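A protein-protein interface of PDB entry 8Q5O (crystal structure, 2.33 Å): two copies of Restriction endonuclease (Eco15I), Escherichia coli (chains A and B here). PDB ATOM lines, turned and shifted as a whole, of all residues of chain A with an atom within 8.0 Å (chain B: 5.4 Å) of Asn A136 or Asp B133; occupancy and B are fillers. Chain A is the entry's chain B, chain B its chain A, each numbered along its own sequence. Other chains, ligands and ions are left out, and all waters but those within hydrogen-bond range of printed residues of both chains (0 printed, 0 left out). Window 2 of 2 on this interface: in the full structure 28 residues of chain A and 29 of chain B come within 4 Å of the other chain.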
ATOM      1  N   ALA A  91       4.271   8.789  -0.922  1.00  0.00           N
ATOM      2  CA  ALA A  91       4.364   7.412  -0.441  1.00  0.00           C
ATOM      3  C   ALA A  91       4.683   7.363   1.056  1.00  0.00           C
ATOM      4  O   ALA A  91       5.600   8.049   1.538  1.00  0.00           O
ATOM      5  CB  ALA A  91       5.432   6.678  -1.232  1.00  0.00           C
ATOM      6  N   LEU A  92       3.932   6.527   1.780  1.00  0.00           N
ATOM      7  CA  LEU A  92       4.327   6.068   3.105  1.00  0.00           C
ATOM      8  C   LEU A  92       5.038   4.709   2.959  1.00  0.00           C
ATOM      9  O   LEU A  92       4.577   3.670   3.443  1.00  0.00           O
ATOM     10  CB  LEU A  92       3.084   6.012   3.999  1.00  0.00           C
ATOM     11  CG  LEU A  92       2.954   7.187   4.960  1.00  0.00           C
ATOM     12  CD1 LEU A  92       2.931   8.496   4.208  1.00  0.00           C
ATOM     13  CD2 LEU A  92       1.725   7.068   5.788  1.00  0.00           C
ATOM     14  N   ARG A  93       6.196   4.739   2.286  1.00  0.00           N
ATOM     15  CA  ARG A  93       6.821   3.497   1.834  1.00  0.00           C
ATOM     16  C   ARG A  93       6.895   2.453   2.949  1.00  0.00           C
ATOM     17  O   ARG A  93       6.671   1.261   2.698  1.00  0.00           O
ATOM     18  CB  ARG A  93       8.226   3.750   1.290  1.00  0.00           C
ATOM     19  CG  ARG A  93       8.251   4.835   0.226  1.00  0.00           C
ATOM     20  CD  ARG A  93       9.451   4.788  -0.692  1.00  0.00           C
ATOM     21  NE  ARG A  93       9.228   3.855  -1.762  1.00  0.00           N
ATOM     22  CZ  ARG A  93       8.938   4.210  -3.011  1.00  0.00           C
ATOM     23  NH1 ARG A  93       8.869   5.483  -3.355  1.00  0.00           N
ATOM     24  NH2 ARG A  93       8.735   3.290  -3.932  1.00  0.00           N
ATOM     25  N   ASN A  94       7.260   2.887   4.162  1.00  0.00           N
ATOM     26  CA  ASN A  94       7.079   2.055   5.340  1.00  0.00           C
ATOM     27  C   ASN A  94       6.103   2.737   6.288  1.00  0.00           C
ATOM     28  O   ASN A  94       6.436   3.757   6.885  1.00  0.00           O
ATOM     29  CB  ASN A  94       8.393   1.727   6.054  1.00  0.00           C
ATOM     30  CG  ASN A  94       8.848   0.298   5.827  1.00  0.00           C
ATOM     31  OD1 ASN A  94       8.231  -0.651   6.310  1.00  0.00           O
ATOM     32  ND2 ASN A  94       9.906   0.131   5.053  1.00  0.00           N
ATOM     33  N   TYR A  95       4.898   2.161   6.379  1.00  0.00           N
ATOM     34  CA  TYR A  95       3.906   2.585   7.349  1.00  0.00           C
ATOM     35  C   TYR A  95       3.626   1.469   8.352  1.00  0.00           C
ATOM     36  O   TYR A  95       3.200   1.763   9.463  1.00  0.00           O
ATOM     37  CB  TYR A  95       2.631   3.036   6.634  1.00  0.00           C
ATOM     38  N   GLU A  96       3.864   0.215   7.963  1.00  0.00           N
ATOM     39  CA  GLU A  96       3.563  -0.934   8.806  1.00  0.00           C
ATOM     40  C   GLU A  96       4.288  -0.817  10.151  1.00  0.00           C
ATOM     41  O   GLU A  96       3.733  -1.197  11.187  1.00  0.00           O
ATOM     42  CB  GLU A  96       3.974  -2.225   8.091  1.00  0.00           C
ATOM     43  CG  GLU A  96       3.412  -2.371   6.691  1.00  0.00           C
ATOM     44  CD  GLU A  96       2.035  -3.018   6.618  1.00  0.00           C
ATOM     45  OE1 GLU A  96       1.137  -2.572   7.358  1.00  0.00           O
ATOM     46  OE2 GLU A  96       1.858  -3.948   5.799  1.00  0.00           O
ATOM     47  N   HIS A 131      -2.140   0.036  -0.958  1.00  0.00           N
ATOM     48  CA  HIS A 131      -0.747  -0.285  -1.181  1.00  0.00           C
ATOM     49  C   HIS A 131      -0.515  -0.478  -2.671  1.00  0.00           C
ATOM     50  O   HIS A 131      -1.225  -1.239  -3.317  1.00  0.00           O
ATOM     51  CB  HIS A 131      -0.331  -1.539  -0.397  1.00  0.00           C
ATOM     52  CG  HIS A 131       0.972  -2.138  -0.852  1.00  0.00           C
ATOM     53  ND1 HIS A 131       1.091  -3.477  -1.168  1.00  0.00           N
ATOM     54  CD2 HIS A 131       2.190  -1.599  -1.081  1.00  0.00           C
ATOM     55  CE1 HIS A 131       2.337  -3.734  -1.558  1.00  0.00           C
ATOM     56  NE2 HIS A 131       3.018  -2.605  -1.535  1.00  0.00           N
ATOM     57  N   SER A 132       0.538   0.179  -3.173  1.00  0.00           N
ATOM     58  CA  SER A 132       0.918   0.107  -4.562  1.00  0.00           C
ATOM     59  C   SER A 132       2.022  -0.930  -4.703  1.00  0.00           C
ATOM     60  O   SER A 132       3.135  -0.696  -4.225  1.00  0.00           O
ATOM     61  CB  SER A 132       1.378   1.443  -5.051  1.00  0.00           C
ATOM     62  OG  SER A 132       2.140   1.301  -6.242  1.00  0.00           O
ATOM     63  N   ASP A 133       1.717  -2.053  -5.366  1.00  0.00           N
ATOM     64  CA  ASP A 133       2.713  -3.089  -5.588  1.00  0.00           C
ATOM     65  C   ASP A 133       3.871  -2.545  -6.423  1.00  0.00           C
ATOM     66  O   ASP A 133       5.008  -3.020  -6.298  1.00  0.00           O
ATOM     67  CB  ASP A 133       2.096  -4.316  -6.260  1.00  0.00           C
ATOM     68  CG  ASP A 133       1.401  -5.239  -5.282  1.00  0.00           C
ATOM     69  OD1 ASP A 133       0.766  -4.735  -4.327  1.00  0.00           O
ATOM     70  OD2 ASP A 133       1.509  -6.449  -5.474  1.00  0.00           O
ATOM     71  N   HIS A 134       3.576  -1.569  -7.291  1.00  0.00           N
ATOM     72  CA  HIS A 134       4.562  -1.056  -8.222  1.00  0.00           C
ATOM     73  C   HIS A 134       5.720  -0.419  -7.453  1.00  0.00           C
ATOM     74  O   HIS A 134       6.874  -0.649  -7.783  1.00  0.00           O
ATOM     75  CB  HIS A 134       3.904  -0.032  -9.152  1.00  0.00           C
ATOM     76  CG  HIS A 134       4.724   0.396 -10.317  1.00  0.00           C
ATOM     77  ND1 HIS A 134       5.242  -0.493 -11.227  1.00  0.00           N
ATOM     78  CD2 HIS A 134       5.027   1.593 -10.777  1.00  0.00           C
ATOM     79  CE1 HIS A 134       5.846   0.166 -12.223  1.00  0.00           C
ATOM     80  NE2 HIS A 134       5.723   1.438 -11.969  1.00  0.00           N
ATOM     81  N   VAL A 135       5.396   0.445  -6.483  1.00  0.00           N
ATOM     82  CA  VAL A 135       6.391   1.267  -5.813  1.00  0.00           C
ATOM     83  C   VAL A 135       6.690   0.737  -4.400  1.00  0.00           C
ATOM     84  O   VAL A 135       7.500   1.313  -3.692  1.00  0.00           O
ATOM     85  CB  VAL A 135       5.942   2.743  -5.753  1.00  0.00           C
ATOM     86  CG1 VAL A 135       5.740   3.333  -7.115  1.00  0.00           C
ATOM     87  CG2 VAL A 135       4.682   2.935  -4.938  1.00  0.00           C
ATOM     88  N   ASN A 136       6.019  -0.335  -3.971  1.00  0.00           N
ATOM     89  CA  ASN A 136       6.183  -0.884  -2.634  1.00  0.00           C
ATOM     90  C   ASN A 136       5.944   0.213  -1.594  1.00  0.00           C
ATOM     91  O   ASN A 136       6.820   0.510  -0.782  1.00  0.00           O
ATOM     92  CB  ASN A 136       7.539  -1.576  -2.490  1.00  0.00           C
ATOM     93  CG  ASN A 136       7.656  -2.393  -1.219  1.00  0.00           C
ATOM     94  OD1 ASN A 136       6.793  -2.312  -0.353  1.00  0.00           O
ATOM     95  ND2 ASN A 136       8.669  -3.242  -1.142  1.00  0.00           N
ATOM     96  N   ALA A 137       4.740   0.782  -1.592  1.00  0.00           N
ATOM     97  CA  ALA A 137       4.421   1.895  -0.718  1.00  0.00           C
ATOM     98  C   ALA A 137       2.902   2.049  -0.595  1.00  0.00           C
ATOM     99  O   ALA A 137       2.155   1.788  -1.539  1.00  0.00           O
ATOM    100  CB  ALA A 137       5.049   3.158  -1.270  1.00  0.00           C
ATOM    101  N   HIS A 138       2.460   2.499   0.582  1.00  0.00           N
ATOM    102  CA  HIS A 138       1.056   2.762   0.842  1.00  0.00           C
ATOM    103  C   HIS A 138       0.726   4.185   0.406  1.00  0.00           C
ATOM    104  O   HIS A 138       1.549   5.099   0.524  1.00  0.00           O
ATOM    105  CB  HIS A 138       0.740   2.574   2.329  1.00  0.00           C
ATOM    106  CG  HIS A 138       1.019   1.191   2.824  1.00  0.00           C
ATOM    107  ND1 HIS A 138       0.308   0.086   2.434  1.00  0.00           N
ATOM    108  CD2 HIS A 138       1.993   0.721   3.596  1.00  0.00           C
ATOM    109  CE1 HIS A 138       0.820  -0.992   2.999  1.00  0.00           C
ATOM    110  NE2 HIS A 138       1.854  -0.636   3.694  1.00  0.00           N
ATOM    111  N   ILE A 139      -0.494   4.345  -0.120  1.00  0.00           N
ATOM    112  CA  ILE A 139      -0.940   5.601  -0.695  1.00  0.00           C
ATOM    113  C   ILE A 139      -2.288   5.978  -0.098  1.00  0.00           C
ATOM    114  O   ILE A 139      -3.151   5.120   0.152  1.00  0.00           O
ATOM    115  CB  ILE A 139      -1.047   5.506  -2.228  1.00  0.00           C
ATOM    116  CG1 ILE A 139       0.133   4.783  -2.876  1.00  0.00           C
ATOM    117  CG2 ILE A 139      -1.241   6.891  -2.820  1.00  0.00           C
ATOM    118  CD1 ILE A 139       1.332   5.673  -3.134  1.00  0.00           C
ATOM    119  N   ARG B 130      21.215  -1.824  -9.833  1.00  0.00           N
ATOM    120  CA  ARG B 130      21.023  -2.631  -8.656  1.00  0.00           C
ATOM    121  C   ARG B 130      19.599  -2.468  -8.237  1.00  0.00           C
ATOM    122  O   ARG B 130      19.003  -1.440  -8.500  1.00  0.00           O
ATOM    123  CB  ARG B 130      21.958  -2.141  -7.550  1.00  0.00           C
ATOM    124  CG  ARG B 130      22.132  -3.078  -6.364  1.00  0.00           C
ATOM    125  CD  ARG B 130      21.073  -2.858  -5.297  1.00  0.00           C
ATOM    126  NE  ARG B 130      20.920  -1.451  -4.952  1.00  0.00           N
ATOM    127  CZ  ARG B 130      20.104  -1.001  -4.008  1.00  0.00           C
ATOM    128  NH1 ARG B 130      19.372  -1.847  -3.302  1.00  0.00           N
ATOM    129  NH2 ARG B 130      20.025   0.294  -3.763  1.00  0.00           N
ATOM    130  N   HIS B 131      19.039  -3.465  -7.581  1.00  0.00           N
ATOM    131  CA  HIS B 131      17.635  -3.382  -7.238  1.00  0.00           C
ATOM    132  C   HIS B 131      17.371  -3.095  -5.784  1.00  0.00           C
ATOM    133  O   HIS B 131      18.030  -3.640  -4.917  1.00  0.00           O
ATOM    134  CB  HIS B 131      16.905  -4.667  -7.611  1.00  0.00           C
ATOM    135  CG  HIS B 131      15.487  -4.700  -7.137  1.00  0.00           C
ATOM    136  ND1 HIS B 131      15.043  -5.581  -6.177  1.00  0.00           N
ATOM    137  CD2 HIS B 131      14.420  -3.938  -7.470  1.00  0.00           C
ATOM    138  CE1 HIS B 131      13.759  -5.373  -5.951  1.00  0.00           C
ATOM    139  NE2 HIS B 131      13.357  -4.379  -6.722  1.00  0.00           N
ATOM    140  N   SER B 132      16.388  -2.250  -5.516  1.00  0.00           N
ATOM    141  CA  SER B 132      16.005  -1.968  -4.154  1.00  0.00           C
ATOM    142  C   SER B 132      14.626  -2.494  -3.913  1.00  0.00           C
ATOM    143  O   SER B 132      13.687  -2.083  -4.573  1.00  0.00           O
ATOM    144  CB  SER B 132      15.989  -0.474  -3.913  1.00  0.00           C
ATOM    145  OG  SER B 132      15.401  -0.171  -2.664  1.00  0.00           O
ATOM    146  N   ASP B 133      14.486  -3.399  -2.962  1.00  0.00           N
ATOM    147  CA  ASP B 133      13.168  -3.891  -2.618  1.00  0.00           C
ATOM    148  C   ASP B 133      12.335  -2.778  -1.991  1.00  0.00           C
ATOM    149  O   ASP B 133      11.131  -2.710  -2.210  1.00  0.00           O
ATOM    150  CB  ASP B 133      13.288  -5.091  -1.682  1.00  0.00           C
ATOM    151  CG  ASP B 133      11.974  -5.823  -1.477  1.00  0.00           C
ATOM    152  OD1 ASP B 133      10.941  -5.165  -1.243  1.00  0.00           O
ATOM    153  OD2 ASP B 133      11.983  -7.070  -1.525  1.00  0.00           O
ATOM    154  N   HIS B 134      12.969  -1.895  -1.236  1.00  0.00           N
ATOM    155  CA  HIS B 134      12.256  -0.819  -0.563  1.00  0.00           C
ATOM    156  C   HIS B 134      11.426   0.046  -1.495  1.00  0.00           C
ATOM    157  O   HIS B 134      10.303   0.393  -1.171  1.00  0.00           O
ATOM    158  CB  HIS B 134      13.275   0.054   0.167  1.00  0.00           C
ATOM    159  CG  HIS B 134      12.675   1.110   1.042  1.00  0.00           C
ATOM    160  ND1 HIS B 134      12.028   0.821   2.222  1.00  0.00           N
ATOM    161  CD2 HIS B 134      12.661   2.458   0.927  1.00  0.00           C
ATOM    162  CE1 HIS B 134      11.622   1.943   2.786  1.00  0.00           C
ATOM    163  NE2 HIS B 134      11.995   2.951   2.021  1.00  0.00           N
ATOM    164  N   VAL B 135      11.977   0.406  -2.640  1.00  0.00           N
ATOM    165  CA  VAL B 135      11.275   1.268  -3.567  1.00  0.00           C
ATOM    166  C   VAL B 135      10.868   0.499  -4.807  1.00  0.00           C
ATOM    167  O   VAL B 135      10.254   1.051  -5.708  1.00  0.00           O
ATOM    168  CB  VAL B 135      12.156   2.446  -3.983  1.00  0.00           C
ATOM    169  CG1 VAL B 135      12.443   3.341  -2.793  1.00  0.00           C
ATOM    170  CG2 VAL B 135      13.441   1.947  -4.618  1.00  0.00           C
ATOM    171  N   ASN B 136      11.198  -0.780  -4.846  1.00  0.00           N
ATOM    172  CA  ASN B 136      10.864  -1.607  -5.997  1.00  0.00           C
ATOM    173  C   ASN B 136      11.342  -0.980  -7.290  1.00  0.00           C
ATOM    174  O   ASN B 136      10.555  -0.748  -8.197  1.00  0.00           O
ATOM    175  CB  ASN B 136       9.362  -1.885  -6.062  1.00  0.00           C
ATOM    176  CG  ASN B 136       8.998  -2.874  -7.152  1.00  0.00           C
ATOM    177  OD1 ASN B 136       9.022  -4.083  -6.941  1.00  0.00           O
ATOM    178  ND2 ASN B 136       8.659  -2.363  -8.326  1.00  0.00           N
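O of Val A135 lies close to O of Val B135 (3.4 Å).
O of Asp B133 lies within hydrogen-bond range of ND2 of Asn A136 (2.7 Å).
The side-chain amide nitrogen (ND2) of Asn B136 lies within hydrogen-bond range of the backbone carbonyl oxygen (O) of His A134 (2.5 Å).
The backbone carbonyl oxygen of Val B135 lies within hydrogen-bond range of the guanidinium group of Arg A93 (3.2 Å).
His A134 touches Asn B136, and with the chains exchanged Asn A136 touches His B134.
Val A135 touches His B134, but with the chains exchanged His A134 does not touch Val B135 (4.3 Å).
Val B135 touches its own counterpart, Val A135.
Asn A136 touches Asp B133, but with the chains exchanged Asp A133 does not touch Asn B136 (4.1 Å).
Positions printed for both chains: 131, 132, 133, 134, 135 and 136.
Of the 8 pairs that touch across the chains among the printed residues, 3 have their exchanged pair printed and touching as well.
Of the 15 printed residues of chain A, 5 touch a printed residue of chain B.
Hydrophobic or aromatic side chains of chain B that line the printed part of chain A: His B134 and Val B135.
Among the printed residues, no Asp or Glu carboxylate lies within 4 Å of a Lys or Arg side-chain nitrogen of the other chain.
Arg A93 touches His B134.
His B134 touches Asn A94 (CE1 to ND2, 3.4 Å).
Val A135 touches His B134 (O to O, 3.9 Å).
His B134 touches Asn A136 (O to O, 3.5 Å).
Of chain B, only Asp B133 (2.7 Å) and His B134 (3.5 Å) come within 4 Å of Asn A136.
Asp B133 touches just one residue of chain A: Asn A136.
No residue of chain A comes within 4 Å of Ser B132.
Of the printed residues of chain B, Val A135 touches His B134 (3.9 Å) and Val B135 (3.4 Å).
Printed residues of chain A within 4 Å of His B134: Arg A93 (3.7 Å), Asn A94 (3.4 Å), Val A135 (3.9 Å) and Asn A136 (3.5 Å).
Printed residues of chain A within 4 Å of Val B135: Arg A93 (3.2 Å) and Val A135 (3.4 Å).
The side-chain hydroxyl (OG) of Ser A132 lies close to the backbone NH (N) of His A134 (3.4 Å).
The backbone NH (N) of Val A135 sits close to the side-chain hydroxyl (OG) of Ser A132, at 3.4 Å.
OG of Ser B132 lies within hydrogen-bond range of N of Val B135 (3.5 Å).
N of His B134 lies close to OG of Ser B132 (3.3 Å).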
